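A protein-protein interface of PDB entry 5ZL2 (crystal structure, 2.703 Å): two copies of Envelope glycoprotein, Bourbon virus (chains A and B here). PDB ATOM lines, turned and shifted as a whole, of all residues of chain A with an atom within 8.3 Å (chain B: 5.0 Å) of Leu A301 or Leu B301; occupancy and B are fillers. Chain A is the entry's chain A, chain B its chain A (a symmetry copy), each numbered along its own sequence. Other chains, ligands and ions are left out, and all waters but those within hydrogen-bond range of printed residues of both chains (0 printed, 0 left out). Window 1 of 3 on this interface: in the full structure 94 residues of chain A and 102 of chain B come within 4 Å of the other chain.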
ATOM      1  N   LEU A 294      22.922  -7.202   3.679  1.00  0.00           N
ATOM      2  CA  LEU A 294      23.473  -8.312   2.911  1.00  0.00           C
ATOM      3  C   LEU A 294      24.221  -9.290   3.811  1.00  0.00           C
ATOM      4  O   LEU A 294      24.097 -10.507   3.645  1.00  0.00           O
ATOM      5  CB  LEU A 294      24.391  -7.787   1.808  1.00  0.00           C
ATOM      6  CG  LEU A 294      25.103  -8.835   0.949  1.00  0.00           C
ATOM      7  CD1 LEU A 294      24.094  -9.685   0.201  1.00  0.00           C
ATOM      8  CD2 LEU A 294      26.069  -8.177  -0.017  1.00  0.00           C
ATOM      9  N   VAL A 295      25.003  -8.777   4.763  1.00  0.00           N
ATOM     10  CA  VAL A 295      25.668  -9.655   5.725  1.00  0.00           C
ATOM     11  C   VAL A 295      24.644 -10.522   6.448  1.00  0.00           C
ATOM     12  O   VAL A 295      24.857 -11.724   6.650  1.00  0.00           O
ATOM     13  CB  VAL A 295      26.510  -8.829   6.718  1.00  0.00           C
ATOM     14  CG1 VAL A 295      26.877  -9.666   7.925  1.00  0.00           C
ATOM     15  CG2 VAL A 295      27.765  -8.291   6.046  1.00  0.00           C
ATOM     16  N   TYR A 296      23.509  -9.928   6.831  1.00  0.00           N
ATOM     17  CA  TYR A 296      22.467 -10.667   7.537  1.00  0.00           C
ATOM     18  C   TYR A 296      21.912 -11.799   6.684  1.00  0.00           C
ATOM     19  O   TYR A 296      21.723 -12.919   7.172  1.00  0.00           O
ATOM     20  CB  TYR A 296      21.347  -9.713   7.949  1.00  0.00           C
ATOM     21  CG  TYR A 296      20.305 -10.311   8.872  1.00  0.00           C
ATOM     22  CD1 TYR A 296      19.156 -10.903   8.366  1.00  0.00           C
ATOM     23  CD2 TYR A 296      20.463 -10.264  10.251  1.00  0.00           C
ATOM     24  CE1 TYR A 296      18.199 -11.440   9.208  1.00  0.00           C
ATOM     25  CE2 TYR A 296      19.514 -10.797  11.098  1.00  0.00           C
ATOM     26  CZ  TYR A 296      18.384 -11.384  10.573  1.00  0.00           C
ATOM     27  OH  TYR A 296      17.438 -11.917  11.417  1.00  0.00           O
ATOM     28  N   GLU A 297      21.638 -11.528   5.408  1.00  0.00           N
ATOM     29  CA  GLU A 297      21.144 -12.577   4.528  1.00  0.00           C
ATOM     30  C   GLU A 297      22.233 -13.566   4.149  1.00  0.00           C
ATOM     31  O   GLU A 297      21.924 -14.719   3.836  1.00  0.00           O
ATOM     32  CB  GLU A 297      20.529 -11.966   3.271  1.00  0.00           C
ATOM     33  CG  GLU A 297      19.267 -11.172   3.544  1.00  0.00           C
ATOM     34  CD  GLU A 297      18.113 -12.057   3.954  1.00  0.00           C
ATOM     35  OE1 GLU A 297      17.555 -12.726   3.065  1.00  0.00           O
ATOM     36  OE2 GLU A 297      17.772 -12.090   5.157  1.00  0.00           O
ATOM     37  N   THR A 298      23.498 -13.147   4.173  1.00  0.00           N
ATOM     38  CA  THR A 298      24.581 -14.084   3.905  1.00  0.00           C
ATOM     39  C   THR A 298      24.755 -15.058   5.060  1.00  0.00           C
ATOM     40  O   THR A 298      24.985 -16.252   4.839  1.00  0.00           O
ATOM     41  CB  THR A 298      25.879 -13.328   3.634  1.00  0.00           C
ATOM     42  OG1 THR A 298      25.710 -12.492   2.485  1.00  0.00           O
ATOM     43  CG2 THR A 298      27.016 -14.298   3.373  1.00  0.00           C
ATOM     44  N   GLU A 299      24.652 -14.571   6.300  1.00  0.00           N
ATOM     45  CA  GLU A 299      24.625 -15.485   7.438  1.00  0.00           C
ATOM     46  C   GLU A 299      23.367 -16.336   7.408  1.00  0.00           C
ATOM     47  O   GLU A 299      23.428 -17.548   7.634  1.00  0.00           O
ATOM     48  CB  GLU A 299      24.714 -14.714   8.757  1.00  0.00           C
ATOM     49  CG  GLU A 299      26.045 -14.008   9.003  1.00  0.00           C
ATOM     50  CD  GLU A 299      27.144 -14.952   9.454  1.00  0.00           C
ATOM     51  OE1 GLU A 299      27.580 -14.850  10.617  1.00  0.00           O
ATOM     52  OE2 GLU A 299      27.579 -15.793   8.642  1.00  0.00           O
ATOM     53  N   SER A 300      22.222 -15.712   7.122  1.00  0.00           N
ATOM     54  CA  SER A 300      20.967 -16.444   7.005  1.00  0.00           C
ATOM     55  C   SER A 300      21.122 -17.650   6.088  1.00  0.00           C
ATOM     56  O   SER A 300      20.834 -18.786   6.474  1.00  0.00           O
ATOM     57  CB  SER A 300      19.876 -15.505   6.483  1.00  0.00           C
ATOM     58  OG  SER A 300      18.585 -15.907   6.908  1.00  0.00           O
ATOM     59  N   LEU A 301      21.606 -17.416   4.868  1.00  0.00           N
ATOM     60  CA  LEU A 301      21.790 -18.499   3.910  1.00  0.00           C
ATOM     61  C   LEU A 301      22.806 -19.525   4.402  1.00  0.00           C
ATOM     62  O   LEU A 301      22.655 -20.721   4.128  1.00  0.00           O
ATOM     63  CB  LEU A 301      22.207 -17.904   2.564  1.00  0.00           C
ATOM     64  CG  LEU A 301      22.465 -18.773   1.331  1.00  0.00           C
ATOM     65  CD1 LEU A 301      23.921 -19.212   1.287  1.00  0.00           C
ATOM     66  CD2 LEU A 301      21.526 -19.972   1.267  1.00  0.00           C
ATOM     67  N   ARG A 302      23.838 -19.088   5.134  1.00  0.00           N
ATOM     68  CA  ARG A 302      24.820 -20.037   5.656  1.00  0.00           C
ATOM     69  C   ARG A 302      24.195 -21.000   6.658  1.00  0.00           C
ATOM     70  O   ARG A 302      24.601 -22.164   6.734  1.00  0.00           O
ATOM     71  CB  ARG A 302      25.989 -19.294   6.301  1.00  0.00           C
ATOM     72  CG  ARG A 302      26.984 -18.728   5.305  1.00  0.00           C
ATOM     73  CD  ARG A 302      27.919 -17.723   5.963  1.00  0.00           C
ATOM     74  NE  ARG A 302      28.906 -18.359   6.830  1.00  0.00           N
ATOM     75  CZ  ARG A 302      30.071 -18.830   6.400  1.00  0.00           C
ATOM     76  NH1 ARG A 302      30.386 -18.741   5.117  1.00  0.00           N
ATOM     77  NH2 ARG A 302      30.920 -19.391   7.248  1.00  0.00           N
ATOM     78  N   LEU A 303      23.212 -20.538   7.431  1.00  0.00           N
ATOM     79  CA  LEU A 303      22.483 -21.440   8.313  1.00  0.00           C
ATOM     80  C   LEU A 303      21.744 -22.502   7.511  1.00  0.00           C
ATOM     81  O   LEU A 303      21.859 -23.701   7.791  1.00  0.00           O
ATOM     82  CB  LEU A 303      21.507 -20.647   9.178  1.00  0.00           C
ATOM     83  CG  LEU A 303      21.978 -20.304  10.590  1.00  0.00           C
ATOM     84  CD1 LEU A 303      20.807 -19.816  11.426  1.00  0.00           C
ATOM     85  CD2 LEU A 303      22.649 -21.503  11.244  1.00  0.00           C
ATOM     86  N   SER A 304      20.976 -22.076   6.503  1.00  0.00           N
ATOM     87  CA  SER A 304      20.212 -23.022   5.695  1.00  0.00           C
ATOM     88  C   SER A 304      21.127 -24.016   4.997  1.00  0.00           C
ATOM     89  O   SER A 304      20.821 -25.213   4.932  1.00  0.00           O
ATOM     90  CB  SER A 304      19.358 -22.276   4.671  1.00  0.00           C
ATOM     91  OG  SER A 304      18.312 -21.565   5.303  1.00  0.00           O
ATOM     92  N   LEU A 305      22.259 -23.543   4.472  1.00  0.00           N
ATOM     93  CA  LEU A 305      23.215 -24.462   3.864  1.00  0.00           C
ATOM     94  C   LEU A 305      23.781 -25.430   4.891  1.00  0.00           C
ATOM     95  O   LEU A 305      24.067 -26.585   4.560  1.00  0.00           O
ATOM     96  CB  LEU A 305      24.349 -23.691   3.195  1.00  0.00           C
ATOM     97  CG  LEU A 305      24.034 -22.954   1.895  1.00  0.00           C
ATOM     98  CD1 LEU A 305      25.330 -22.566   1.209  1.00  0.00           C
ATOM     99  CD2 LEU A 305      23.156 -23.787   0.971  1.00  0.00           C
ATOM    100  N   ALA A 306      23.955 -24.979   6.135  1.00  0.00           N
ATOM    101  CA  ALA A 306      24.465 -25.869   7.171  1.00  0.00           C
ATOM    102  C   ALA A 306      23.429 -26.918   7.551  1.00  0.00           C
ATOM    103  O   ALA A 306      23.769 -28.087   7.754  1.00  0.00           O
ATOM    104  CB  ALA A 306      24.891 -25.061   8.394  1.00  0.00           C
ATOM    105  N   GLN A 307      22.161 -26.520   7.653  1.00  0.00           N
ATOM    106  CA  GLN A 307      21.113 -27.487   7.956  1.00  0.00           C
ATOM    107  C   GLN A 307      21.012 -28.538   6.860  1.00  0.00           C
ATOM    108  O   GLN A 307      20.777 -29.717   7.141  1.00  0.00           O
ATOM    109  CB  GLN A 307      19.776 -26.769   8.148  1.00  0.00           C
ATOM    110  CG  GLN A 307      18.578 -27.690   8.291  1.00  0.00           C
ATOM    111  CD  GLN A 307      17.309 -26.937   8.643  1.00  0.00           C
ATOM    112  OE1 GLN A 307      17.344 -25.740   8.925  1.00  0.00           O
ATOM    113  NE2 GLN A 307      16.181 -27.638   8.641  1.00  0.00           N
ATOM    114  N   LEU A 308      21.203 -28.134   5.603  1.00  0.00           N
ATOM    115  CA  LEU A 308      21.131 -29.088   4.501  1.00  0.00           C
ATOM    116  C   LEU A 308      22.334 -30.022   4.495  1.00  0.00           C
ATOM    117  O   LEU A 308      22.208 -31.202   4.149  1.00  0.00           O
ATOM    118  CB  LEU A 308      21.023 -28.345   3.170  1.00  0.00           C
ATOM    119  CG  LEU A 308      19.645 -27.791   2.801  1.00  0.00           C
ATOM    120  CD1 LEU A 308      19.641 -27.299   1.368  1.00  0.00           C
ATOM    121  CD2 LEU A 308      18.571 -28.842   3.004  1.00  0.00           C
ATOM    122  N   LEU A 404      17.849 -28.425 -11.028  1.00  0.00           N
ATOM    123  CA  LEU A 404      17.796 -27.500  -9.906  1.00  0.00           C
ATOM    124  C   LEU A 404      17.835 -26.063 -10.402  1.00  0.00           C
ATOM    125  O   LEU A 404      18.731 -25.685 -11.163  1.00  0.00           O
ATOM    126  CB  LEU A 404      18.960 -27.755  -8.952  1.00  0.00           C
ATOM    127  CG  LEU A 404      19.096 -26.761  -7.800  1.00  0.00           C
ATOM    128  CD1 LEU A 404      17.897 -26.858  -6.872  1.00  0.00           C
ATOM    129  CD2 LEU A 404      20.397 -26.995  -7.038  1.00  0.00           C
ATOM    130  N   TRP A 405      16.859 -25.267  -9.972  1.00  0.00           N
ATOM    131  CA  TRP A 405      16.881 -23.846 -10.283  1.00  0.00           C
ATOM    132  C   TRP A 405      18.054 -23.179  -9.576  1.00  0.00           C
ATOM    133  O   TRP A 405      18.290 -23.412  -8.386  1.00  0.00           O
ATOM    134  CB  TRP A 405      15.580 -23.176  -9.862  1.00  0.00           C
ATOM    135  CG  TRP A 405      15.737 -21.694  -9.800  1.00  0.00           C
ATOM    136  CD1 TRP A 405      15.845 -20.924  -8.678  1.00  0.00           C
ATOM    137  CD2 TRP A 405      15.833 -20.800 -10.911  1.00  0.00           C
ATOM    138  NE1 TRP A 405      15.994 -19.602  -9.024  1.00  0.00           N
ATOM    139  CE2 TRP A 405      15.989 -19.501 -10.390  1.00  0.00           C
ATOM    140  CE3 TRP A 405      15.794 -20.973 -12.298  1.00  0.00           C
ATOM    141  CZ2 TRP A 405      16.106 -18.381 -11.205  1.00  0.00           C
ATOM    142  CZ3 TRP A 405      15.912 -19.859 -13.108  1.00  0.00           C
ATOM    143  CH2 TRP A 405      16.068 -18.579 -12.558  1.00  0.00           C
ATOM    144  N   LEU A 406      18.789 -22.347 -10.309  1.00  0.00           N
ATOM    145  CA  LEU A 406      19.924 -21.635  -9.756  1.00  0.00           C
ATOM    146  C   LEU A 406      19.710 -20.136  -9.892  1.00  0.00           C
ATOM    147  O   LEU A 406      19.339 -19.664 -10.978  1.00  0.00           O
ATOM    148  CB  LEU A 406      21.223 -22.035 -10.457  1.00  0.00           C
ATOM    149  CG  LEU A 406      21.683 -23.469 -10.258  1.00  0.00           C
ATOM    150  CD1 LEU A 406      22.721 -23.800 -11.296  1.00  0.00           C
ATOM    151  CD2 LEU A 406      22.251 -23.627  -8.872  1.00  0.00           C
ATOM    152  N   PRO A 407      19.919 -19.361  -8.831  1.00  0.00           N
ATOM    153  CA  PRO A 407      19.817 -17.901  -8.949  1.00  0.00           C
ATOM    154  C   PRO A 407      20.839 -17.371  -9.942  1.00  0.00           C
ATOM    155  O   PRO A 407      22.048 -17.539  -9.767  1.00  0.00           O
ATOM    156  CB  PRO A 407      20.097 -17.414  -7.522  1.00  0.00           C
ATOM    157  CG  PRO A 407      19.822 -18.603  -6.644  1.00  0.00           C
ATOM    158  CD  PRO A 407      20.215 -19.793  -7.455  1.00  0.00           C
ATOM    159  N   GLN A 408      20.342 -16.740 -11.000  1.00  0.00           N
ATOM    160  CA  GLN A 408      21.215 -16.219 -12.036  1.00  0.00           C
ATOM    161  C   GLN A 408      21.894 -14.938 -11.565  1.00  0.00           C
ATOM    162  O   GLN A 408      21.425 -14.258 -10.649  1.00  0.00           O
ATOM    163  CB  GLN A 408      20.427 -15.957 -13.316  1.00  0.00           C
ATOM    164  CG  GLN A 408      19.590 -17.140 -13.762  1.00  0.00           C
ATOM    165  CD  GLN A 408      19.472 -17.227 -15.267  1.00  0.00           C
ATOM    166  OE1 GLN A 408      18.372 -17.323 -15.811  1.00  0.00           O
ATOM    167  NE2 GLN A 408      20.611 -17.185 -15.951  1.00  0.00           N
ATOM    168  N   GLU B 297      29.186 -13.130  -4.124  1.00  0.00           N
ATOM    169  CA  GLU B 297      28.426 -14.023  -3.261  1.00  0.00           C
ATOM    170  C   GLU B 297      27.347 -14.773  -4.023  1.00  0.00           C
ATOM    171  O   GLU B 297      26.953 -15.863  -3.600  1.00  0.00           O
ATOM    172  CB  GLU B 297      27.806 -13.240  -2.107  1.00  0.00           C
ATOM    173  CG  GLU B 297      28.831 -12.677  -1.142  1.00  0.00           C
ATOM    174  CD  GLU B 297      29.516 -13.759  -0.340  1.00  0.00           C
ATOM    175  OE1 GLU B 297      28.871 -14.289   0.583  1.00  0.00           O
ATOM    176  OE2 GLU B 297      30.687 -14.084  -0.636  1.00  0.00           O
ATOM    177  N   THR B 298      26.864 -14.220  -5.136  1.00  0.00           N
ATOM    178  CA  THR B 298      25.894 -14.945  -5.946  1.00  0.00           C
ATOM    179  C   THR B 298      26.551 -16.111  -6.668  1.00  0.00           C
ATOM    180  O   THR B 298      25.968 -17.196  -6.760  1.00  0.00           O
ATOM    181  CB  THR B 298      25.227 -13.999  -6.942  1.00  0.00           C
ATOM    182  OG1 THR B 298      24.539 -12.968  -6.229  1.00  0.00           O
ATOM    183  CG2 THR B 298      24.230 -14.750  -7.804  1.00  0.00           C
ATOM    184  N   GLU B 299      27.766 -15.911  -7.188  1.00  0.00           N
ATOM    185  CA  GLU B 299      28.519 -17.039  -7.726  1.00  0.00           C
ATOM    186  C   GLU B 299      28.891 -18.009  -6.617  1.00  0.00           C
ATOM    187  O   GLU B 299      28.760 -19.225  -6.782  1.00  0.00           O
ATOM    188  CB  GLU B 299      29.777 -16.557  -8.452  1.00  0.00           C
ATOM    189  CG  GLU B 299      29.519 -15.765  -9.732  1.00  0.00           C
ATOM    190  CD  GLU B 299      29.147 -16.644 -10.911  1.00  0.00           C
ATOM    191  OE1 GLU B 299      29.946 -16.737 -11.864  1.00  0.00           O
ATOM    192  OE2 GLU B 299      28.050 -17.239 -10.890  1.00  0.00           O
ATOM    193  N   SER B 300      29.347 -17.480  -5.480  1.00  0.00           N
ATOM    194  CA  SER B 300      29.671 -18.315  -4.330  1.00  0.00           C
ATOM    195  C   SER B 300      28.530 -19.275  -4.014  1.00  0.00           C
ATOM    196  O   SER B 300      28.721 -20.493  -3.954  1.00  0.00           O
ATOM    197  CB  SER B 300      29.977 -17.425  -3.122  1.00  0.00           C
ATOM    198  OG  SER B 300      30.857 -18.059  -2.209  1.00  0.00           O
ATOM    199  N   LEU B 301      27.326 -18.735  -3.834  1.00  0.00           N
ATOM    200  CA  LEU B 301      26.167 -19.563  -3.522  1.00  0.00           C
ATOM    201  C   LEU B 301      25.851 -20.542  -4.650  1.00  0.00           C
ATOM    202  O   LEU B 301      25.403 -21.663  -4.384  1.00  0.00           O
ATOM    203  CB  LEU B 301      24.975 -18.654  -3.222  1.00  0.00           C
ATOM    204  CG  LEU B 301      23.601 -19.208  -2.840  1.00  0.00           C
ATOM    205  CD1 LEU B 301      22.762 -19.451  -4.086  1.00  0.00           C
ATOM    206  CD2 LEU B 301      23.706 -20.471  -1.991  1.00  0.00           C
ATOM    207  N   ARG B 302      26.081 -20.147  -5.909  1.00  0.00           N
ATOM    208  CA  ARG B 302      25.824 -21.060  -7.021  1.00  0.00           C
ATOM    209  C   ARG B 302      26.737 -22.279  -6.970  1.00  0.00           C
ATOM    210  O   ARG B 302      26.326 -23.377  -7.362  1.00  0.00           O
ATOM    211  CB  ARG B 302      25.989 -20.335  -8.356  1.00  0.00           C
ATOM    212  CG  ARG B 302      24.808 -19.458  -8.730  1.00  0.00           C
ATOM    213  CD  ARG B 302      25.160 -18.510  -9.867  1.00  0.00           C
ATOM    214  NE  ARG B 302      25.266 -19.191 -11.154  1.00  0.00           N
ATOM    215  CZ  ARG B 302      24.234 -19.419 -11.956  1.00  0.00           C
ATOM    216  NH1 ARG B 302      23.021 -19.026 -11.598  1.00  0.00           N
ATOM    217  NH2 ARG B 302      24.409 -20.040 -13.114  1.00  0.00           N
ATOM    218  N   LEU B 303      27.971 -22.110  -6.496  1.00  0.00           N
ATOM    219  CA  LEU B 303      28.846 -23.258  -6.296  1.00  0.00           C
ATOM    220  C   LEU B 303      28.266 -24.209  -5.258  1.00  0.00           C
ATOM    221  O   LEU B 303      28.159 -25.416  -5.498  1.00  0.00           O
ATOM    222  CB  LEU B 303      30.234 -22.786  -5.873  1.00  0.00           C
ATOM    223  CG  LEU B 303      31.285 -22.692  -6.978  1.00  0.00           C
ATOM    224  CD1 LEU B 303      32.669 -22.533  -6.370  1.00  0.00           C
ATOM    225  CD2 LEU B 303      31.228 -23.913  -7.885  1.00  0.00           C
ATOM    226  N   SER B 304      27.885 -23.675  -4.094  1.00  0.00           N
ATOM    227  CA  SER B 304      27.340 -24.516  -3.031  1.00  0.00           C
ATOM    228  C   SER B 304      26.073 -25.225  -3.485  1.00  0.00           C
ATOM    229  O   SER B 304      25.875 -26.409  -3.187  1.00  0.00           O
ATOM    230  CB  SER B 304      27.063 -23.679  -1.783  1.00  0.00           C
ATOM    231  OG  SER B 304      28.268 -23.246  -1.184  1.00  0.00           O
ATOM    232  N   LEU B 305      25.202 -24.520  -4.211  1.00  0.00           N
ATOM    233  CA  LEU B 305      24.011 -25.171  -4.744  1.00  0.00           C
ATOM    234  C   LEU B 305      24.374 -26.258  -5.742  1.00  0.00           C
ATOM    235  O   LEU B 305      23.680 -27.276  -5.829  1.00  0.00           O
ATOM    236  CB  LEU B 305      23.089 -24.147  -5.401  1.00  0.00           C
ATOM    237  CG  LEU B 305      22.320 -23.197  -4.486  1.00  0.00           C
ATOM    238  CD1 LEU B 305      21.214 -22.523  -5.275  1.00  0.00           C
ATOM    239  CD2 LEU B 305      21.757 -23.917  -3.267  1.00  0.00           C
ATOM    240  N   ALA B 306      25.450 -26.060  -6.507  1.00  0.00           N
ATOM    241  CA  ALA B 306      25.867 -27.080  -7.461  1.00  0.00           C
ATOM    242  C   ALA B 306      26.430 -28.301  -6.748  1.00  0.00           C
ATOM    243  O   ALA B 306      26.157 -29.438  -7.144  1.00  0.00           O
ATOM    244  CB  ALA B 306      26.891 -26.502  -8.435  1.00  0.00           C
ATOM    245  N   PRO B 407      16.092 -17.954   4.381  1.00  0.00           N
ATOM    246  CA  PRO B 407      16.394 -16.524   4.528  1.00  0.00           C
ATOM    247  C   PRO B 407      15.194 -15.680   4.129  1.00  0.00           C
ATOM    248  O   PRO B 407      14.723 -15.736   2.990  1.00  0.00           O
ATOM    249  CB  PRO B 407      17.582 -16.317   3.583  1.00  0.00           C
ATOM    250  CG  PRO B 407      18.168 -17.688   3.388  1.00  0.00           C
ATOM    251  CD  PRO B 407      17.009 -18.626   3.446  1.00  0.00           C
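The guanidinium group of Arg B302 sits at hydrogen-bond distance from the backbone carbonyl oxygen of Pro A407 (2.6 Å).
Among the printed residues, merely in contact across the chains: Ser A300 with Pro B407 (3.3 Å), Thr A298 with Glu B297 (3.4 Å), Gln A408 with Arg B302 (3.4 Å), Leu A404 with Leu B305 (3.5 Å), Leu A301 with Leu B301 (3.5 Å), Leu A406 with Leu B305 (3.6 Å), Glu A297 with Pro B407 (3.6 Å), Leu A305 with Ser B304 (3.6 Å), Pro A407 with Leu B305 (3.6 Å), Leu A406 with Arg B302 (3.7 Å), Ser A304 with Pro B407 (3.7 Å), Leu A301 with Pro B407 (3.7 Å) and Pro A407 with Leu B301 (3.99 Å).
Thr A298 touches Glu B297, but with the chains exchanged Glu A297 does not touch Thr B298 (10.3 Å).
Leu B301 touches its own counterpart, Leu A301.
Leu A305 touches Ser B304, but with the chains exchanged Ser A304 does not touch Leu B305 (8.3 Å).
Pro A407 touches Leu B305, but with the chains exchanged Leu A305 does not touch Pro B407 (7.2 Å).
Positions printed for both chains: 297, 298, 299, 300, 301, 302, 303, 304, 305, 306 and 407.
Of the 14 pairs that touch across the chains among the printed residues, 3 have their exchanged pair printed and touching as well.
Leu A294 touches none of the printed residues of chain B.
Printed residues of chain B within 4 Å of Ser A300: Pro B407.
Leu A301 touches just these residues of chain B: Leu B301 (3.5 Å) and Pro B407 (3.7 Å).
Arg A302 touches none of the printed residues of chain B.
Of the printed residues of chain B, Ser A304 touches Pro B407 (3.7 Å).
Printed residues of chain B within 4 Å of Leu A305: Ser B304 (3.6 Å).
Of the printed residues of chain B, Leu A406 touches Arg B302 and Leu B305.
Printed residues of chain A within 4 Å of Leu B301: Leu A301 (3.5 Å) and Pro A407 (3.99 Å).
The nearest printed residue of chain A that does not touch Leu B301 is Leu A305 (4.2 Å).
Hydrophobic or aromatic side chains of chain B within 4 Å of the printed part of chain A: Leu B301, Leu B305 and Pro B407.
Of the 20 printed residues of chain A, 10 touch a printed residue of chain B.
Along chain A the printed residues that touch a printed residue of chain B span positions 297 to 408.
Among the printed residues, no Asp or Glu carboxylate lies within 4 Å of a Lys or Arg side-chain nitrogen of the other chain.
O of Leu A294 lies within hydrogen-bond range of OG1 of Thr A298 (2.8 Å).
The side-chain carboxylate of Glu B299 is in salt-bridge range of the guanidinium group of Arg B302, at 3.4 Å.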
